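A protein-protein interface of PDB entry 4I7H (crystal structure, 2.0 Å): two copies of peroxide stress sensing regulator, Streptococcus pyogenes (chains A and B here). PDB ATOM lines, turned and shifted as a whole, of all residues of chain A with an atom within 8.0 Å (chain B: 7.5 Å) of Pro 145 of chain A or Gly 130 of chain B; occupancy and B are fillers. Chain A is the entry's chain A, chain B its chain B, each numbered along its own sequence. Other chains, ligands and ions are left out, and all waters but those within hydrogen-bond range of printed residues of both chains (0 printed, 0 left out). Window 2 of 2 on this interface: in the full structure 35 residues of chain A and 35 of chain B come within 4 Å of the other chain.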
ATOM      1  N   VAL A 102      10.144 -25.617  10.906  1.00  0.00           N
ATOM      2  CA  VAL A 102       9.674 -26.317  12.093  1.00  0.00           C
ATOM      3  C   VAL A 102       8.239 -25.905  12.311  1.00  0.00           C
ATOM      4  O   VAL A 102       7.907 -24.723  12.200  1.00  0.00           O
ATOM      5  CB  VAL A 102      10.463 -25.956  13.337  1.00  0.00           C
ATOM      6  CG1 VAL A 102      10.175 -26.933  14.468  1.00  0.00           C
ATOM      7  CG2 VAL A 102      11.935 -25.910  13.016  1.00  0.00           C
ATOM      8  N   CYS A 104       5.000 -25.937  14.912  1.00  0.00           N
ATOM      9  CA  CYS A 104       4.555 -26.155  16.290  1.00  0.00           C
ATOM     10  C   CYS A 104       3.343 -27.082  16.334  1.00  0.00           C
ATOM     11  O   CYS A 104       2.334 -26.824  15.672  1.00  0.00           O
ATOM     12  CB  CYS A 104       4.208 -24.850  16.996  1.00  0.00           C
ATOM     13  SG  CYS A 104       3.439 -25.208  18.595  1.00  0.00           S
ATOM     14  N   CYS A 107      -0.124 -25.087  18.067  1.00  0.00           N
ATOM     15  CA  CYS A 107      -0.748 -23.941  17.419  1.00  0.00           C
ATOM     16  C   CYS A 107      -0.516 -23.866  15.911  1.00  0.00           C
ATOM     17  O   CYS A 107      -1.210 -23.117  15.217  1.00  0.00           O
ATOM     18  CB  CYS A 107      -0.269 -22.650  18.083  1.00  0.00           C
ATOM     19  SG  CYS A 107       1.276 -22.019  17.415  1.00  0.00           S
ATOM     20  N   LYS A 109       2.170 -22.694  14.259  1.00  0.00           N
ATOM     21  CA  LYS A 109       3.092 -21.640  13.814  1.00  0.00           C
ATOM     22  C   LYS A 109       4.343 -22.239  13.176  1.00  0.00           C
ATOM     23  O   LYS A 109       4.957 -23.153  13.728  1.00  0.00           O
ATOM     24  CB  LYS A 109       3.493 -20.714  14.977  1.00  0.00           C
ATOM     25  CG  LYS A 109       4.619 -19.719  14.637  1.00  0.00           C
ATOM     26  CD  LYS A 109       4.798 -18.639  15.719  1.00  0.00           C
ATOM     27  CE  LYS A 109       5.987 -18.925  16.646  1.00  0.00           C
ATOM     28  NZ  LYS A 109       5.784 -18.361  18.036  1.00  0.00           N
ATOM     29  N   ALA A 111       8.243 -21.704  11.701  1.00  0.00           N
ATOM     30  CA  ALA A 111       9.463 -20.918  11.607  1.00  0.00           C
ATOM     31  C   ALA A 111      10.433 -21.735  10.773  1.00  0.00           C
ATOM     32  O   ALA A 111      10.220 -22.931  10.575  1.00  0.00           O
ATOM     33  CB  ALA A 111      10.033 -20.652  12.988  1.00  0.00           C
ATOM     34  N   PHE A 113      14.783 -22.565   9.840  1.00  0.00           N
ATOM     35  CA  PHE A 113      16.154 -22.440  10.316  1.00  0.00           C
ATOM     36  C   PHE A 113      17.125 -22.822   9.212  1.00  0.00           C
ATOM     37  O   PHE A 113      16.764 -23.513   8.256  1.00  0.00           O
ATOM     38  CB  PHE A 113      16.379 -23.274  11.582  1.00  0.00           C
ATOM     39  CG  PHE A 113      16.168 -24.749  11.382  1.00  0.00           C
ATOM     40  CD1 PHE A 113      17.243 -25.593  11.168  1.00  0.00           C
ATOM     41  CD2 PHE A 113      14.893 -25.286  11.399  1.00  0.00           C
ATOM     42  CE1 PHE A 113      17.051 -26.949  10.978  1.00  0.00           C
ATOM     43  CE2 PHE A 113      14.698 -26.646  11.217  1.00  0.00           C
ATOM     44  CZ  PHE A 113      15.776 -27.471  11.013  1.00  0.00           C
ATOM     45  N   GLY A 142       7.874 -29.364  16.743  1.00  0.00           N
ATOM     46  CA  GLY A 142       8.208 -29.071  18.118  1.00  0.00           C
ATOM     47  C   GLY A 142       7.220 -28.150  18.792  1.00  0.00           C
ATOM     48  O   GLY A 142       6.093 -27.966  18.319  1.00  0.00           O
ATOM     49  N   ILE A 143       7.645 -27.575  19.912  1.00  0.00           N
ATOM     50  CA  ILE A 143       6.801 -26.656  20.670  1.00  0.00           C
ATOM     51  C   ILE A 143       7.377 -25.242  20.560  1.00  0.00           C
ATOM     52  O   ILE A 143       8.509 -24.995  20.991  1.00  0.00           O
ATOM     53  CB  ILE A 143       6.707 -27.074  22.155  1.00  0.00           C
ATOM     54  CG1 ILE A 143       6.286 -28.548  22.270  1.00  0.00           C
ATOM     55  CG2 ILE A 143       5.731 -26.164  22.903  1.00  0.00           C
ATOM     56  CD1 ILE A 143       4.875 -28.834  21.751  1.00  0.00           C
ATOM     57  N   CYS A 144       6.615 -24.330  19.961  1.00  0.00           N
ATOM     58  CA  CYS A 144       7.099 -22.967  19.739  1.00  0.00           C
ATOM     59  C   CYS A 144       7.200 -22.222  21.078  1.00  0.00           C
ATOM     60  O   CYS A 144       6.506 -22.570  22.039  1.00  0.00           O
ATOM     61  CB  CYS A 144       6.164 -22.215  18.796  1.00  0.00           C
ATOM     62  SG  CYS A 144       4.903 -21.274  19.684  1.00  0.00           S
ATOM     63  N   PRO A 145       8.073 -21.200  21.144  1.00  0.00           N
ATOM     64  CA  PRO A 145       8.318 -20.467  22.394  1.00  0.00           C
ATOM     65  C   PRO A 145       7.041 -19.952  23.056  1.00  0.00           C
ATOM     66  O   PRO A 145       6.899 -20.090  24.273  1.00  0.00           O
ATOM     67  CB  PRO A 145       9.204 -19.306  21.943  1.00  0.00           C
ATOM     68  CG  PRO A 145       9.929 -19.848  20.736  1.00  0.00           C
ATOM     69  CD  PRO A 145       8.905 -20.694  20.036  1.00  0.00           C
ATOM     70  N   ASP A 146       6.120 -19.399  22.271  1.00  0.00           N
ATOM     71  CA  ASP A 146       4.854 -18.904  22.814  1.00  0.00           C
ATOM     72  C   ASP A 146       3.981 -19.995  23.438  1.00  0.00           C
ATOM     73  O   ASP A 146       3.282 -19.746  24.420  1.00  0.00           O
ATOM     74  CB  ASP A 146       4.052 -18.157  21.744  1.00  0.00           C
ATOM     75  CG  ASP A 146       4.563 -16.749  21.512  1.00  0.00           C
ATOM     76  OD1 ASP A 146       5.379 -16.272  22.336  1.00  0.00           O
ATOM     77  OD2 ASP A 146       4.142 -16.116  20.514  1.00  0.00           O
ATOM     78  N   CYS A 147       4.017 -21.199  22.872  1.00  0.00           N
ATOM     79  CA  CYS A 147       3.194 -22.290  23.391  1.00  0.00           C
ATOM     80  C   CYS A 147       3.796 -22.951  24.620  1.00  0.00           C
ATOM     81  O   CYS A 147       3.087 -23.594  25.397  1.00  0.00           O
ATOM     82  CB  CYS A 147       2.908 -23.328  22.311  1.00  0.00           C
ATOM     83  SG  CYS A 147       1.360 -23.028  21.457  1.00  0.00           S
ATOM     84  N   GLN A 148       5.102 -22.797  24.798  1.00  0.00           N
ATOM     85  CA  GLN A 148       5.742 -23.290  26.007  1.00  0.00           C
ATOM     86  C   GLN A 148       5.922 -22.166  27.035  1.00  0.00           C
ATOM     87  O   GLN A 148       5.016 -21.354  27.249  1.00  0.00           O
ATOM     88  CB  GLN A 148       7.075 -23.967  25.683  1.00  0.00           C
ATOM     89  CG  GLN A 148       8.022 -23.125  24.837  1.00  0.00           C
ATOM     90  CD  GLN A 148       9.194 -23.931  24.293  1.00  0.00           C
ATOM     91  OE1 GLN A 148       9.774 -24.756  24.997  1.00  0.00           O
ATOM     92  NE2 GLN A 148       9.548 -23.693  23.036  1.00  0.00           N
ATOM     93  N   THR B  42      16.926 -30.471  24.927  1.00  0.00           N
ATOM     94  CA  THR B  42      17.450 -29.280  24.277  1.00  0.00           C
ATOM     95  C   THR B  42      18.978 -29.225  24.444  1.00  0.00           C
ATOM     96  O   THR B  42      19.739 -29.280  23.462  1.00  0.00           O
ATOM     97  CB  THR B  42      16.790 -28.019  24.894  1.00  0.00           C
ATOM     98  OG1 THR B  42      15.572 -27.713  24.194  1.00  0.00           O
ATOM     99  CG2 THR B  42      17.730 -26.821  24.856  1.00  0.00           C
ATOM    100  N   GLU B 124      20.372 -27.461  15.815  1.00  0.00           N
ATOM    101  CA  GLU B 124      20.348 -26.240  15.014  1.00  0.00           C
ATOM    102  C   GLU B 124      18.957 -25.600  15.016  1.00  0.00           C
ATOM    103  O   GLU B 124      18.844 -24.376  15.102  1.00  0.00           O
ATOM    104  CB  GLU B 124      20.855 -26.460  13.586  1.00  0.00           C
ATOM    105  CG  GLU B 124      22.378 -26.327  13.434  1.00  0.00           C
ATOM    106  CD  GLU B 124      22.961 -25.122  14.186  1.00  0.00           C
ATOM    107  OE1 GLU B 124      22.405 -23.999  14.077  1.00  0.00           O
ATOM    108  OE2 GLU B 124      23.985 -25.302  14.894  1.00  0.00           O
ATOM    109  N   ALA B 125      17.907 -26.418  14.968  1.00  0.00           N
ATOM    110  CA  ALA B 125      16.553 -25.884  15.014  1.00  0.00           C
ATOM    111  C   ALA B 125      16.295 -25.197  16.352  1.00  0.00           C
ATOM    112  O   ALA B 125      15.814 -24.072  16.384  1.00  0.00           O
ATOM    113  CB  ALA B 125      15.519 -26.963  14.769  1.00  0.00           C
ATOM    114  N   HIS B 126      16.627 -25.860  17.457  1.00  0.00           N
ATOM    115  CA  HIS B 126      16.373 -25.260  18.756  1.00  0.00           C
ATOM    116  C   HIS B 126      17.169 -23.971  18.971  1.00  0.00           C
ATOM    117  O   HIS B 126      16.625 -22.998  19.489  1.00  0.00           O
ATOM    118  CB  HIS B 126      16.641 -26.226  19.905  1.00  0.00           C
ATOM    119  CG  HIS B 126      16.399 -25.611  21.249  1.00  0.00           C
ATOM    120  ND1 HIS B 126      15.137 -25.479  21.791  1.00  0.00           N
ATOM    121  CD2 HIS B 126      17.249 -25.034  22.129  1.00  0.00           C
ATOM    122  CE1 HIS B 126      15.226 -24.879  22.965  1.00  0.00           C
ATOM    123  NE2 HIS B 126      16.497 -24.595  23.192  1.00  0.00           N
ATOM    124  N   GLU B 127      18.441 -23.969  18.574  1.00  0.00           N
ATOM    125  CA  GLU B 127      19.307 -22.796  18.716  1.00  0.00           C
ATOM    126  C   GLU B 127      18.778 -21.561  17.976  1.00  0.00           C
ATOM    127  O   GLU B 127      18.835 -20.440  18.492  1.00  0.00           O
ATOM    128  CB  GLU B 127      20.727 -23.101  18.210  1.00  0.00           C
ATOM    129  CG  GLU B 127      21.596 -23.975  19.125  1.00  0.00           C
ATOM    130  CD  GLU B 127      22.998 -24.182  18.548  1.00  0.00           C
ATOM    131  OE1 GLU B 127      23.546 -23.222  17.957  1.00  0.00           O
ATOM    132  OE2 GLU B 127      23.550 -25.302  18.670  1.00  0.00           O
ATOM    133  N   GLN B 128      18.260 -21.764  16.771  1.00  0.00           N
ATOM    134  CA  GLN B 128      17.877 -20.647  15.914  1.00  0.00           C
ATOM    135  C   GLN B 128      16.448 -20.161  16.102  1.00  0.00           C
ATOM    136  O   GLN B 128      16.112 -19.027  15.744  1.00  0.00           O
ATOM    137  CB  GLN B 128      18.057 -21.040  14.450  1.00  0.00           C
ATOM    138  CG  GLN B 128      19.496 -21.233  14.047  1.00  0.00           C
ATOM    139  CD  GLN B 128      19.620 -21.640  12.603  1.00  0.00           C
ATOM    140  OE1 GLN B 128      19.027 -21.014  11.717  1.00  0.00           O
ATOM    141  NE2 GLN B 128      20.386 -22.711  12.350  1.00  0.00           N
ATOM    142  N   THR B 129      15.602 -21.008  16.669  1.00  0.00           N
ATOM    143  CA  THR B 129      14.175 -20.806  16.529  1.00  0.00           C
ATOM    144  C   THR B 129      13.484 -20.815  17.889  1.00  0.00           C
ATOM    145  O   THR B 129      12.370 -20.316  18.038  1.00  0.00           O
ATOM    146  CB  THR B 129      13.598 -21.899  15.594  1.00  0.00           C
ATOM    147  OG1 THR B 129      12.555 -21.366  14.770  1.00  0.00           O
ATOM    148  CG2 THR B 129      13.085 -23.059  16.382  1.00  0.00           C
ATOM    149  N   GLY B 130      14.156 -21.385  18.882  1.00  0.00           N
ATOM    150  CA  GLY B 130      13.592 -21.486  20.211  1.00  0.00           C
ATOM    151  C   GLY B 130      12.563 -22.589  20.403  1.00  0.00           C
ATOM    152  O   GLY B 130      12.098 -22.813  21.530  1.00  0.00           O
ATOM    153  N   TYR B 131      12.183 -23.276  19.328  1.00  0.00           N
ATOM    154  CA  TYR B 131      11.218 -24.370  19.471  1.00  0.00           C
ATOM    155  C   TYR B 131      11.847 -25.486  20.306  1.00  0.00           C
ATOM    156  O   TYR B 131      13.045 -25.738  20.219  1.00  0.00           O
ATOM    157  CB  TYR B 131      10.791 -24.950  18.107  1.00  0.00           C
ATOM    158  CG  TYR B 131       9.769 -24.148  17.316  1.00  0.00           C
ATOM    159  CD1 TYR B 131       9.950 -22.793  17.068  1.00  0.00           C
ATOM    160  CD2 TYR B 131       8.637 -24.758  16.790  1.00  0.00           C
ATOM    161  CE1 TYR B 131       9.030 -22.065  16.322  1.00  0.00           C
ATOM    162  CE2 TYR B 131       7.711 -24.038  16.046  1.00  0.00           C
ATOM    163  CZ  TYR B 131       7.918 -22.688  15.816  1.00  0.00           C
ATOM    164  OH  TYR B 131       7.013 -21.962  15.080  1.00  0.00           O
ATOM    165  N   LYS B 132      11.042 -26.126  21.138  1.00  0.00           N
ATOM    166  CA  LYS B 132      11.458 -27.360  21.769  1.00  0.00           C
ATOM    167  C   LYS B 132      11.175 -28.456  20.744  1.00  0.00           C
ATOM    168  O   LYS B 132      10.022 -28.736  20.455  1.00  0.00           O
ATOM    169  CB  LYS B 132      10.648 -27.603  23.045  1.00  0.00           C
ATOM    170  CG  LYS B 132      10.998 -28.891  23.785  1.00  0.00           C
ATOM    171  CD  LYS B 132      12.496 -28.987  24.070  1.00  0.00           C
ATOM    172  CE  LYS B 132      12.790 -29.922  25.241  1.00  0.00           C
ATOM    173  NZ  LYS B 132      13.244 -29.173  26.459  1.00  0.00           N
ATOM    174  N   VAL B 133      12.215 -29.057  20.179  1.00  0.00           N
ATOM    175  CA  VAL B 133      12.010 -30.028  19.094  1.00  0.00           C
ATOM    176  C   VAL B 133      11.434 -31.346  19.625  1.00  0.00           C
ATOM    177  O   VAL B 133      11.988 -31.949  20.544  1.00  0.00           O
ATOM    178  CB  VAL B 133      13.301 -30.263  18.295  1.00  0.00           C
ATOM    179  CG1 VAL B 133      13.051 -31.248  17.124  1.00  0.00           C
ATOM    180  CG2 VAL B 133      13.828 -28.944  17.776  1.00  0.00           C
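OH of Tyr 131 of chain B is in hydrogen-bond range of O of Lys 109 of chain A, 2.7 Å away.
The backbone carbonyl oxygen (O) of Lys 132 of chain B is in hydrogen-bond range of the backbone NH (N) of Ile 143 of chain A (2.7 Å).
The side-chain amide nitrogen (NE2) of Gln 148 of chain A sits at hydrogen-bond distance from the backbone carbonyl oxygen (O) of Gly 130 of chain B.
The side-chain amide nitrogen of Gln 148 of chain A sits close to the backbone NH of Lys 132 of chain B, 3.4 Å away.
The backbone carbonyl oxygen (O) of Lys 109 of chain A lies within hydrogen-bond range of the backbone NH (N) of Cys 104 of chain A.
The side-chain sulfur of Cys 107 of chain A sits close to the backbone NH of Lys 109 of chain A.
The side-chain sulfur (SG) of Cys 144 of chain A lies close to the side-chain amino group (NZ) of Lys 109 of chain A.
OD2 of Asp 146 of chain A is in salt-bridge range of NZ of Lys 109 of chain A, at 3.7 Å.
The backbone carbonyl oxygen (O) of Ile 143 of chain A is in hydrogen-bond range of the side-chain amide nitrogen (NE2) of Gln 148 of chain A (2.6 Å).
SG of Cys 144 of chain A sits close to N of Asp 146 of chain A.
Among the printed residues, merely in contact across the chains: Val 102 of chain A with Tyr 131 of chain B (3.5 Å), Cys 104 of chain A with Tyr 131 of chain B (3.5 Å), Ala 111 of chain A with Thr 129 of chain B (3.2 Å), Ala 111 of chain A with Tyr 131 of chain B (3.6 Å), Phe 113 of chain A with Ala 125 of chain B (3.7 Å), Phe 113 of chain A with Gln 128 of chain B (3.5 Å), Gly 142 of chain A with Lys 132 of chain B (3.0 Å), Ile 143 of chain A with Tyr 131 of chain B (3.2 Å), Cys 144 of chain A with Tyr 131 of chain B (3.5 Å), Pro 145 of chain A with Thr 129 of chain B (3.7 Å), Pro 145 of chain A with Gly 130 of chain B (3.8 Å), Pro 145 of chain A with Tyr 131 of chain B (3.8 Å) and Gln 148 of chain A with Tyr 131 of chain B (3.99 Å).
Of chain B, only Thr 129 (3.7 Å), Gly 130 (3.8 Å) and Tyr 131 (3.8 Å) come within 4 Å of Pro 145 of chain A.
Printed residues of chain B within 4 Å of Cys 104 of chain A: Tyr 131.
Of the printed residues of chain A, Tyr 131 of chain B touches Val 102, Cys 104, Lys 109, Ala 111, Ile 143, Cys 144, Pro 145 and Gln 148.
Of the printed residues of chain A, Ala 125 of chain B touches Phe 113 (3.7 Å).
Of the printed residues of chain B, Cys 144 of chain A touches Tyr 131.
Of the printed residues of chain A, Lys 132 of chain B touches Gly 142 (3.0 Å), Ile 143 (2.7 Å) and Gln 148 (3.4 Å).
His 126 of chain B touches none of the printed residues of chain A.
Glu 124 of chain B touches none of the printed residues of chain A.
The nearest printed residue of chain B that does not touch Cys 144 of chain A is Lys 132 of chain B (4.9 Å).
Hydrophobic or aromatic side chains of chain B within 4 Å of the printed part of chain A: Ala 125 and Tyr 131.
Of the 13 printed residues of chain A, 10 touch a printed residue of chain B.
Hydrophobic or aromatic side chains of chain A within 4 Å of the printed part of chain B: Val 102, Ala 111, Phe 113 and Pro 145.
No position is printed for both chains.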
